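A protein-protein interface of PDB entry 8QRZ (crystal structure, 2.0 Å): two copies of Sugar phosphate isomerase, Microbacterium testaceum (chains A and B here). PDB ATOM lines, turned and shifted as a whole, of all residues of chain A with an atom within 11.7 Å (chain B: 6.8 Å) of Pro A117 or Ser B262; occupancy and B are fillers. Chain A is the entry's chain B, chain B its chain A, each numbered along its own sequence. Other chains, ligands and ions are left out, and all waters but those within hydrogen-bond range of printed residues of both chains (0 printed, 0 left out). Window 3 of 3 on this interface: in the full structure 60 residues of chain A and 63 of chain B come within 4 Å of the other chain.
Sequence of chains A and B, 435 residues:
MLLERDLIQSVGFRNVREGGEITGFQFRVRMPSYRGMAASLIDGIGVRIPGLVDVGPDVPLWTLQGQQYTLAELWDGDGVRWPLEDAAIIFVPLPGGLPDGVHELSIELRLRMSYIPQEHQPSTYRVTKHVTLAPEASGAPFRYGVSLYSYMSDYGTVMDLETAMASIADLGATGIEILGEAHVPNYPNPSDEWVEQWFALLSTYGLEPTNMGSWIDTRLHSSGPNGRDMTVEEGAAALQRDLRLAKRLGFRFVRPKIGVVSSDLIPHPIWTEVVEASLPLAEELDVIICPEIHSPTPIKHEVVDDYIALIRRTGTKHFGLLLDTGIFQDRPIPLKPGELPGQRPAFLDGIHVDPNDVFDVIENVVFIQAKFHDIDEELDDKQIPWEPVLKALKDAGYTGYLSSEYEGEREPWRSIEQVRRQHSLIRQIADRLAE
Leu A111 touches none of the printed residues of chain B. Of the printed residues of chain B, Ser A114 touches Arg B219 and Val B260. Printed residues of chain B within 4 Å of Ile A116: Arg B219 (2.8 Å) and Val B260 (3.8 Å). Of the printed residues of chain B, Gln A118 touches Arg B219. Of the printed residues of chain B, Gln A121 touches Arg B219 (3.8 Å). Ser A123 touches none of the printed residues of chain B. Of the printed residues of chain A, Val B260 touches Ser A114, Tyr A115, Ile A116 and Pro A117. Ser B262 touches just one residue of chain A: Pro A117 (3.8 Å). Ser B263 touches one residue of chain A. No residue of chain A comes within 4 Å of Asp B264. Of chain A, only Tyr A115 and Pro A117 come within 4 Å of Leu B265. No residue of chain A comes within 4 Å of Ile B266. The nearest printed residue of chain B that does not touch Arg A112 is Val B260 (10.0 Å).
Among the printed residues, pairs that only touch across the chains: Tyr A115 with Val B260, Tyr A115 with Leu B265, Gln A118 with Arg B219, Pro A117 with Leu B265, Ile A116 with Val B260, Pro A117 with Ser B263, Pro A117 with Ser B262, Pro A117 with Val B260 and Gln A121 with Arg B219.
No position is printed for both chains. Of the 14 pairs that touch across the chains among the printed residues, none has its exchanged pair printed and touching as well.
Of the 10 printed residues of chain B, 5 touch a printed residue of chain A. Hydrophobic or aromatic side chains of chain B within 4 Å of the printed part of chain A: Val B260 and Leu B265. Among the printed residues, no Asp or Glu carboxylate lies within 4 Å of a Lys or Arg side-chain nitrogen of the other chain.
The side-chain hydroxyl of Ser B262 is in hydrogen-bond range of the side-chain carboxylate of Asp B264 (3.3 Å). OH of Tyr A34 lies within hydrogen-bond range of OH of Tyr A115 (2.5 Å). OD1 of Asp A43 lies within salt-bridge range of NH1 of Arg A112, 2.8 Å away. OE1 of Gln A121 lies close to O of Leu A111 (3.3 Å). The side-chain amide oxygen of Gln A121 lies within hydrogen-bond range of the backbone NH of Met A113 (2.8 Å). NE2 of Gln A121 lies within hydrogen-bond range of OG of Ser A123, 2.9 Å away.
The backbone carbonyl oxygen (O) of Arg B219 is in hydrogen-bond range of the guanidinium group (NH2) of Arg A112. The backbone carbonyl oxygen (O) of Met A113 is in hydrogen-bond range of the guanidinium group (NH1) of Arg B219. The backbone NH (N) of Arg B219 sits at hydrogen-bond distance from the side-chain hydroxyl (OG) of Ser A114 (3.1 Å). The backbone carbonyl oxygen (O) of Ile A116 lies within hydrogen-bond range of the guanidinium group (NH1) of Arg B219 (2.8 Å). N of Val B260 is in hydrogen-bond range of O of Ser A114 (2.9 Å).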
ATOM      1  N   TYR A  34     -20.184 -21.299   9.578  1.00  0.00           N
ATOM      2  CA  TYR A  34     -20.498 -21.299   8.161  1.00  0.00           C
ATOM      3  C   TYR A  34     -19.260 -21.366   7.281  1.00  0.00           C
ATOM      4  O   TYR A  34     -19.408 -21.407   6.061  1.00  0.00           O
ATOM      5  CB  TYR A  34     -21.347 -20.085   7.788  1.00  0.00           C
ATOM      6  CG  TYR A  34     -21.054 -18.842   8.559  1.00  0.00           C
ATOM      7  CD1 TYR A  34     -19.898 -18.119   8.318  1.00  0.00           C
ATOM      8  CD2 TYR A  34     -21.943 -18.374   9.525  1.00  0.00           C
ATOM      9  CE1 TYR A  34     -19.617 -16.977   9.024  1.00  0.00           C
ATOM     10  CE2 TYR A  34     -21.669 -17.220  10.233  1.00  0.00           C
ATOM     11  CZ  TYR A  34     -20.506 -16.528   9.971  1.00  0.00           C
ATOM     12  OH  TYR A  34     -20.216 -15.373  10.653  1.00  0.00           O
ATOM     13  N   ASP A  43     -10.790 -23.105  20.228  1.00  0.00           N
ATOM     14  CA  ASP A  43     -10.495 -22.948  21.644  1.00  0.00           C
ATOM     15  C   ASP A  43     -10.747 -24.232  22.432  1.00  0.00           C
ATOM     16  O   ASP A  43     -10.768 -24.196  23.663  1.00  0.00           O
ATOM     17  CB  ASP A  43     -11.315 -21.802  22.232  1.00  0.00           C
ATOM     18  CG  ASP A  43     -10.468 -20.603  22.609  1.00  0.00           C
ATOM     19  OD1 ASP A  43      -9.295 -20.495  22.160  1.00  0.00           O
ATOM     20  OD2 ASP A  43     -10.986 -19.774  23.385  1.00  0.00           O
ATOM     21  N   LEU A 111     -15.108 -21.910  19.604  1.00  0.00           N
ATOM     22  CA  LEU A 111     -14.492 -21.338  18.413  1.00  0.00           C
ATOM     23  C   LEU A 111     -14.343 -19.831  18.605  1.00  0.00           C
ATOM     24  O   LEU A 111     -15.203 -19.188  19.206  1.00  0.00           O
ATOM     25  CB  LEU A 111     -15.339 -21.608  17.139  1.00  0.00           C
ATOM     26  CG  LEU A 111     -15.513 -23.031  16.576  1.00  0.00           C
ATOM     27  CD1 LEU A 111     -16.206 -22.978  15.213  1.00  0.00           C
ATOM     28  CD2 LEU A 111     -14.164 -23.766  16.464  1.00  0.00           C
ATOM     29  N   ARG A 112     -13.260 -19.262  18.075  1.00  0.00           N
ATOM     30  CA  ARG A 112     -13.006 -17.826  18.172  1.00  0.00           C
ATOM     31  C   ARG A 112     -13.321 -17.182  16.829  1.00  0.00           C
ATOM     32  O   ARG A 112     -12.596 -17.401  15.852  1.00  0.00           O
ATOM     33  CB  ARG A 112     -11.560 -17.541  18.568  1.00  0.00           C
ATOM     34  CG  ARG A 112     -11.163 -18.026  19.934  1.00  0.00           C
ATOM     35  CD  ARG A 112      -9.885 -17.331  20.419  1.00  0.00           C
ATOM     36  NE  ARG A 112      -8.802 -17.310  19.445  1.00  0.00           N
ATOM     37  CZ  ARG A 112      -8.012 -18.351  19.190  1.00  0.00           C
ATOM     38  NH1 ARG A 112      -8.233 -19.539  19.736  1.00  0.00           N
ATOM     39  NH2 ARG A 112      -6.980 -18.202  18.362  1.00  0.00           N
ATOM     40  N   MET A 113     -14.403 -16.391  16.782  1.00  0.00           N
ATOM     41  CA  MET A 113     -14.744 -15.584  15.617  1.00  0.00           C
ATOM     42  C   MET A 113     -14.350 -14.144  15.933  1.00  0.00           C
ATOM     43  O   MET A 113     -14.954 -13.513  16.809  1.00  0.00           O
ATOM     44  CB  MET A 113     -16.232 -15.671  15.298  1.00  0.00           C
ATOM     45  CG  MET A 113     -16.926 -16.827  15.990  1.00  0.00           C
ATOM     46  SD  MET A 113     -16.404 -18.470  15.469  1.00  0.00           S
ATOM     47  CE  MET A 113     -17.467 -18.803  14.065  1.00  0.00           C
ATOM     48  N   SER A 114     -13.359 -13.615  15.206  1.00  0.00           N
ATOM     49  CA  SER A 114     -12.823 -12.286  15.529  1.00  0.00           C
ATOM     50  C   SER A 114     -13.840 -11.162  15.305  1.00  0.00           C
ATOM     51  O   SER A 114     -13.747 -10.109  15.943  1.00  0.00           O
ATOM     52  CB  SER A 114     -11.564 -12.011  14.708  1.00  0.00           C
ATOM     53  OG  SER A 114     -10.656 -13.101  14.734  1.00  0.00           O
ATOM     54  N   TYR A 115     -14.793 -11.346  14.408  1.00  0.00           N
ATOM     55  CA  TYR A 115     -15.744 -10.302  14.070  1.00  0.00           C
ATOM     56  C   TYR A 115     -16.875 -10.171  15.082  1.00  0.00           C
ATOM     57  O   TYR A 115     -17.793  -9.371  14.871  1.00  0.00           O
ATOM     58  CB  TYR A 115     -16.332 -10.577  12.686  1.00  0.00           C
ATOM     59  CG  TYR A 115     -16.815 -12.011  12.498  1.00  0.00           C
ATOM     60  CD1 TYR A 115     -15.956 -13.012  12.049  1.00  0.00           C
ATOM     61  CD2 TYR A 115     -18.125 -12.361  12.777  1.00  0.00           C
ATOM     62  CE1 TYR A 115     -16.400 -14.307  11.880  1.00  0.00           C
ATOM     63  CE2 TYR A 115     -18.575 -13.663  12.609  1.00  0.00           C
ATOM     64  CZ  TYR A 115     -17.710 -14.630  12.163  1.00  0.00           C
ATOM     65  OH  TYR A 115     -18.177 -15.925  11.999  1.00  0.00           O
ATOM     66  N   ILE A 116     -16.859 -10.960  16.148  1.00  0.00           N
ATOM     67  CA  ILE A 116     -17.910 -10.891  17.155  1.00  0.00           C
ATOM     68  C   ILE A 116     -17.304 -10.279  18.409  1.00  0.00           C
ATOM     69  O   ILE A 116     -16.152 -10.589  18.746  1.00  0.00           O
ATOM     70  CB  ILE A 116     -18.522 -12.271  17.423  1.00  0.00           C
ATOM     71  CG1 ILE A 116     -19.187 -12.812  16.158  1.00  0.00           C
ATOM     72  CG2 ILE A 116     -19.492 -12.207  18.568  1.00  0.00           C
ATOM     73  CD1 ILE A 116     -20.391 -12.012  15.718  1.00  0.00           C
ATOM     74  N   PRO A 117     -18.030  -9.401  19.108  1.00  0.00           N
ATOM     75  CA  PRO A 117     -17.479  -8.752  20.311  1.00  0.00           C
ATOM     76  C   PRO A 117     -16.996  -9.740  21.373  1.00  0.00           C
ATOM     77  O   PRO A 117     -17.620 -10.775  21.622  1.00  0.00           O
ATOM     78  CB  PRO A 117     -18.660  -7.919  20.825  1.00  0.00           C
ATOM     79  CG  PRO A 117     -19.458  -7.609  19.599  1.00  0.00           C
ATOM     80  CD  PRO A 117     -19.328  -8.820  18.703  1.00  0.00           C
ATOM     81  N   GLN A 118     -15.886  -9.377  22.027  1.00  0.00           N
ATOM     82  CA  GLN A 118     -15.263 -10.233  23.045  1.00  0.00           C
ATOM     83  C   GLN A 118     -16.250 -10.704  24.107  1.00  0.00           C
ATOM     84  O   GLN A 118     -16.151 -11.834  24.601  1.00  0.00           O
ATOM     85  CB  GLN A 118     -14.106  -9.491  23.720  1.00  0.00           C
ATOM     86  CG  GLN A 118     -12.826  -9.525  22.922  1.00  0.00           C
ATOM     87  CD  GLN A 118     -11.732 -10.250  23.660  1.00  0.00           C
ATOM     88  OE1 GLN A 118     -11.939 -10.710  24.786  1.00  0.00           O
ATOM     89  NE2 GLN A 118     -10.564 -10.388  23.022  1.00  0.00           N
ATOM     90  N   GLU A 119     -17.200  -9.850  24.485  1.00  0.00           N
ATOM     91  CA  GLU A 119     -18.135 -10.196  25.546  1.00  0.00           C
ATOM     92  C   GLU A 119     -19.080 -11.322  25.134  1.00  0.00           C
ATOM     93  O   GLU A 119     -19.827 -11.841  25.979  1.00  0.00           O
ATOM     94  CB  GLU A 119     -18.900  -8.932  25.967  1.00  0.00           C
ATOM     95  CG  GLU A 119     -18.006  -7.868  26.651  1.00  0.00           C
ATOM     96  CD  GLU A 119     -17.479  -6.823  25.671  1.00  0.00           C
ATOM     97  OE1 GLU A 119     -17.686  -6.997  24.445  1.00  0.00           O
ATOM     98  OE2 GLU A 119     -16.866  -5.822  26.117  1.00  0.00           O
ATOM     99  N   HIS A 120     -19.042 -11.732  23.862  1.00  0.00           N
ATOM    100  CA  HIS A 120     -19.875 -12.810  23.347  1.00  0.00           C
ATOM    101  C   HIS A 120     -19.035 -13.956  22.780  1.00  0.00           C
ATOM    102  O   HIS A 120     -19.522 -14.746  21.969  1.00  0.00           O
ATOM    103  CB  HIS A 120     -20.845 -12.252  22.303  1.00  0.00           C
ATOM    104  CG  HIS A 120     -21.889 -11.347  22.880  1.00  0.00           C
ATOM    105  ND1 HIS A 120     -22.087 -10.055  22.434  1.00  0.00           N
ATOM    106  CD2 HIS A 120     -22.789 -11.545  23.874  1.00  0.00           C
ATOM    107  CE1 HIS A 120     -23.066  -9.497  23.125  1.00  0.00           C
ATOM    108  NE2 HIS A 120     -23.506 -10.378  24.007  1.00  0.00           N
ATOM    109  N   GLN A 121     -17.790 -14.080  23.222  1.00  0.00           N
ATOM    110  CA  GLN A 121     -16.856 -15.067  22.718  1.00  0.00           C
ATOM    111  C   GLN A 121     -16.167 -15.762  23.883  1.00  0.00           C
ATOM    112  O   GLN A 121     -16.065 -15.193  24.976  1.00  0.00           O
ATOM    113  CB  GLN A 121     -15.809 -14.407  21.810  1.00  0.00           C
ATOM    114  CG  GLN A 121     -16.352 -13.975  20.476  1.00  0.00           C
ATOM    115  CD  GLN A 121     -16.649 -15.154  19.570  1.00  0.00           C
ATOM    116  OE1 GLN A 121     -15.746 -15.918  19.194  1.00  0.00           O
ATOM    117  NE2 GLN A 121     -17.915 -15.321  19.233  1.00  0.00           N
ATOM    118  N   PRO A 122     -15.676 -16.998  23.683  1.00  0.00           N
ATOM    119  CA  PRO A 122     -15.701 -17.764  22.433  1.00  0.00           C
ATOM    120  C   PRO A 122     -17.089 -18.240  22.060  1.00  0.00           C
ATOM    121  O   PRO A 122     -17.944 -18.367  22.941  1.00  0.00           O
ATOM    122  CB  PRO A 122     -14.795 -18.957  22.739  1.00  0.00           C
ATOM    123  CG  PRO A 122     -14.947 -19.165  24.181  1.00  0.00           C
ATOM    124  CD  PRO A 122     -15.062 -17.775  24.777  1.00  0.00           C
ATOM    125  N   SER A 123     -17.303 -18.454  20.763  1.00  0.00           N
ATOM    126  CA  SER A 123     -18.526 -19.082  20.287  1.00  0.00           C
ATOM    127  C   SER A 123     -18.571 -20.514  20.793  1.00  0.00           C
ATOM    128  O   SER A 123     -17.577 -21.237  20.702  1.00  0.00           O
ATOM    129  CB  SER A 123     -18.577 -19.052  18.758  1.00  0.00           C
ATOM    130  OG  SER A 123     -19.069 -17.810  18.279  1.00  0.00           O
ATOM    131  N   THR A 124     -19.710 -20.930  21.328  1.00  0.00           N
ATOM    132  CA  THR A 124     -19.797 -22.212  22.006  1.00  0.00           C
ATOM    133  C   THR A 124     -20.979 -23.020  21.488  1.00  0.00           C
ATOM    134  O   THR A 124     -22.052 -22.480  21.215  1.00  0.00           O
ATOM    135  CB  THR A 124     -19.876 -21.998  23.526  1.00  0.00           C
ATOM    136  OG1 THR A 124     -18.713 -21.268  23.942  1.00  0.00           O
ATOM    137  CG2 THR A 124     -19.889 -23.299  24.261  1.00  0.00           C
ATOM    138  N   ARG B 219      -7.909 -12.163  15.710  1.00  0.00           N
ATOM    139  CA  ARG B 219      -7.667 -12.959  16.909  1.00  0.00           C
ATOM    140  C   ARG B 219      -7.019 -14.307  16.600  1.00  0.00           C
ATOM    141  O   ARG B 219      -7.038 -15.204  17.450  1.00  0.00           O
ATOM    142  CB  ARG B 219      -8.964 -13.168  17.690  1.00  0.00           C
ATOM    143  CG  ARG B 219      -9.749 -11.904  17.894  1.00  0.00           C
ATOM    144  CD  ARG B 219     -10.756 -12.062  19.017  1.00  0.00           C
ATOM    145  NE  ARG B 219     -11.458 -10.809  19.246  1.00  0.00           N
ATOM    146  CZ  ARG B 219     -12.774 -10.660  19.215  1.00  0.00           C
ATOM    147  NH1 ARG B 219     -13.583 -11.696  19.077  1.00  0.00           N
ATOM    148  NH2 ARG B 219     -13.291  -9.440  19.335  1.00  0.00           N
ATOM    149  N   VAL B 260     -13.197  -7.322  15.254  1.00  0.00           N
ATOM    150  CA  VAL B 260     -13.755  -6.131  15.881  1.00  0.00           C
ATOM    151  C   VAL B 260     -13.178  -5.936  17.278  1.00  0.00           C
ATOM    152  O   VAL B 260     -12.544  -6.821  17.848  1.00  0.00           O
ATOM    153  CB  VAL B 260     -15.283  -6.194  15.943  1.00  0.00           C
ATOM    154  CG1 VAL B 260     -15.829  -6.580  14.578  1.00  0.00           C
ATOM    155  CG2 VAL B 260     -15.691  -7.188  17.017  1.00  0.00           C
ATOM    156  N   VAL B 261     -13.417  -4.745  17.837  1.00  0.00           N
ATOM    157  CA  VAL B 261     -12.895  -4.376  19.146  1.00  0.00           C
ATOM    158  C   VAL B 261     -13.957  -3.809  20.082  1.00  0.00           C
ATOM    159  O   VAL B 261     -13.637  -3.472  21.224  1.00  0.00           O
ATOM    160  CB  VAL B 261     -11.726  -3.380  19.004  1.00  0.00           C
ATOM    161  CG1 VAL B 261     -10.799  -3.811  17.904  1.00  0.00           C
ATOM    162  CG2 VAL B 261     -12.263  -2.005  18.684  1.00  0.00           C
ATOM    163  N   SER B 262     -15.213  -3.706  19.651  1.00  0.00           N
ATOM    164  CA  SER B 262     -16.241  -3.029  20.434  1.00  0.00           C
ATOM    165  C   SER B 262     -17.612  -3.540  20.014  1.00  0.00           C
ATOM    166  O   SER B 262     -17.756  -4.240  19.006  1.00  0.00           O
ATOM    167  CB  SER B 262     -16.170  -1.516  20.251  1.00  0.00           C
ATOM    168  OG  SER B 262     -16.626  -1.191  18.950  1.00  0.00           O
ATOM    169  N   SER B 263     -18.631  -3.125  20.778  1.00  0.00           N
ATOM    170  CA  SER B 263     -19.964  -3.719  20.671  1.00  0.00           C
ATOM    171  C   SER B 263     -20.601  -3.444  19.317  1.00  0.00           C
ATOM    172  O   SER B 263     -21.176  -4.350  18.696  1.00  0.00           O
ATOM    173  CB  SER B 263     -20.864  -3.187  21.782  1.00  0.00           C
ATOM    174  OG  SER B 263     -20.127  -2.979  22.965  1.00  0.00           O
ATOM    175  N   ASP B 264     -20.543  -2.192  18.856  1.00  0.00           N
ATOM    176  CA  ASP B 264     -21.114  -1.855  17.557  1.00  0.00           C
ATOM    177  C   ASP B 264     -20.065  -2.060  16.470  1.00  0.00           C
ATOM    178  O   ASP B 264     -20.099  -1.406  15.421  1.00  0.00           O
ATOM    179  CB  ASP B 264     -21.679  -0.425  17.536  1.00  0.00           C
ATOM    180  CG  ASP B 264     -20.749   0.603  18.174  1.00  0.00           C
ATOM    181  OD1 ASP B 264     -19.633   0.240  18.624  1.00  0.00           O
ATOM    182  OD2 ASP B 264     -21.140   1.791  18.205  1.00  0.00           O
ATOM    183  N   LEU B 265     -19.124  -2.974  16.735  1.00  0.00           N
ATOM    184  CA  LEU B 265     -18.306  -3.619  15.705  1.00  0.00           C
ATOM    185  C   LEU B 265     -17.362  -2.619  15.024  1.00  0.00           C
ATOM    186  O   LEU B 265     -17.334  -2.494  13.798  1.00  0.00           O
ATOM    187  CB  LEU B 265     -19.188  -4.345  14.674  1.00  0.00           C
ATOM    188  CG  LEU B 265     -20.287  -5.326  15.125  1.00  0.00           C
ATOM    189  CD1 LEU B 265     -21.153  -5.720  13.961  1.00  0.00           C
ATOM    190  CD2 LEU B 265     -19.702  -6.572  15.750  1.00  0.00           C
ATOM    191  N   ILE B 266     -16.575  -1.913  15.828  1.00  0.00           N
ATOM    192  CA  ILE B 266     -15.507  -1.084  15.263  1.00  0.00           C
ATOM    193  C   ILE B 266     -14.299  -1.949  14.911  1.00  0.00           C
ATOM    194  O   ILE B 266     -13.715  -2.593  15.795  1.00  0.00           O
ATOM    195  CB  ILE B 266     -15.113   0.067  16.202  1.00  0.00           C
ATOM    196  CG1 ILE B 266     -16.285   1.043  16.378  1.00  0.00           C
ATOM    197  CG2 ILE B 266     -13.901   0.789  15.654  1.00  0.00           C
ATOM    198  CD1 ILE B 266     -16.397   1.630  17.756  1.00  0.00           C
ATOM    199  N   PRO B 267     -13.900  -1.993  13.637  1.00  0.00           N
ATOM    200  CA  PRO B 267     -12.804  -2.883  13.226  1.00  0.00           C
ATOM    201  C   PRO B 267     -11.511  -2.607  13.976  1.00  0.00           C
ATOM    202  O   PRO B 267     -11.292  -1.531  14.531  1.00  0.00           O
ATOM    203  CB  PRO B 267     -12.643  -2.599  11.726  1.00  0.00           C
ATOM    204  CG  PRO B 267     -13.706  -1.570  11.362  1.00  0.00           C
ATOM    205  CD  PRO B 267     -14.663  -1.460  12.495  1.00  0.00           C
ATOM    206  N   HIS B 301     -22.876   6.126  11.002  1.00  0.00           N
ATOM    207  CA  HIS B 301     -22.035   5.559  12.056  1.00  0.00           C
ATOM    208  C   HIS B 301     -20.569   5.785  11.710  1.00  0.00           C
ATOM    209  O   HIS B 301     -20.196   5.813  10.533  1.00  0.00           O
ATOM    210  CB  HIS B 301     -22.313   4.060  12.244  1.00  0.00           C
ATOM    211  CG  HIS B 301     -21.707   3.484  13.484  1.00  0.00           C
ATOM    212  ND1 HIS B 301     -20.375   3.145  13.576  1.00  0.00           N
ATOM    213  CD2 HIS B 301     -22.254   3.194  14.689  1.00  0.00           C
ATOM    214  CE1 HIS B 301     -20.125   2.665  14.782  1.00  0.00           C
ATOM    215  NE2 HIS B 301     -21.249   2.692  15.480  1.00  0.00           N
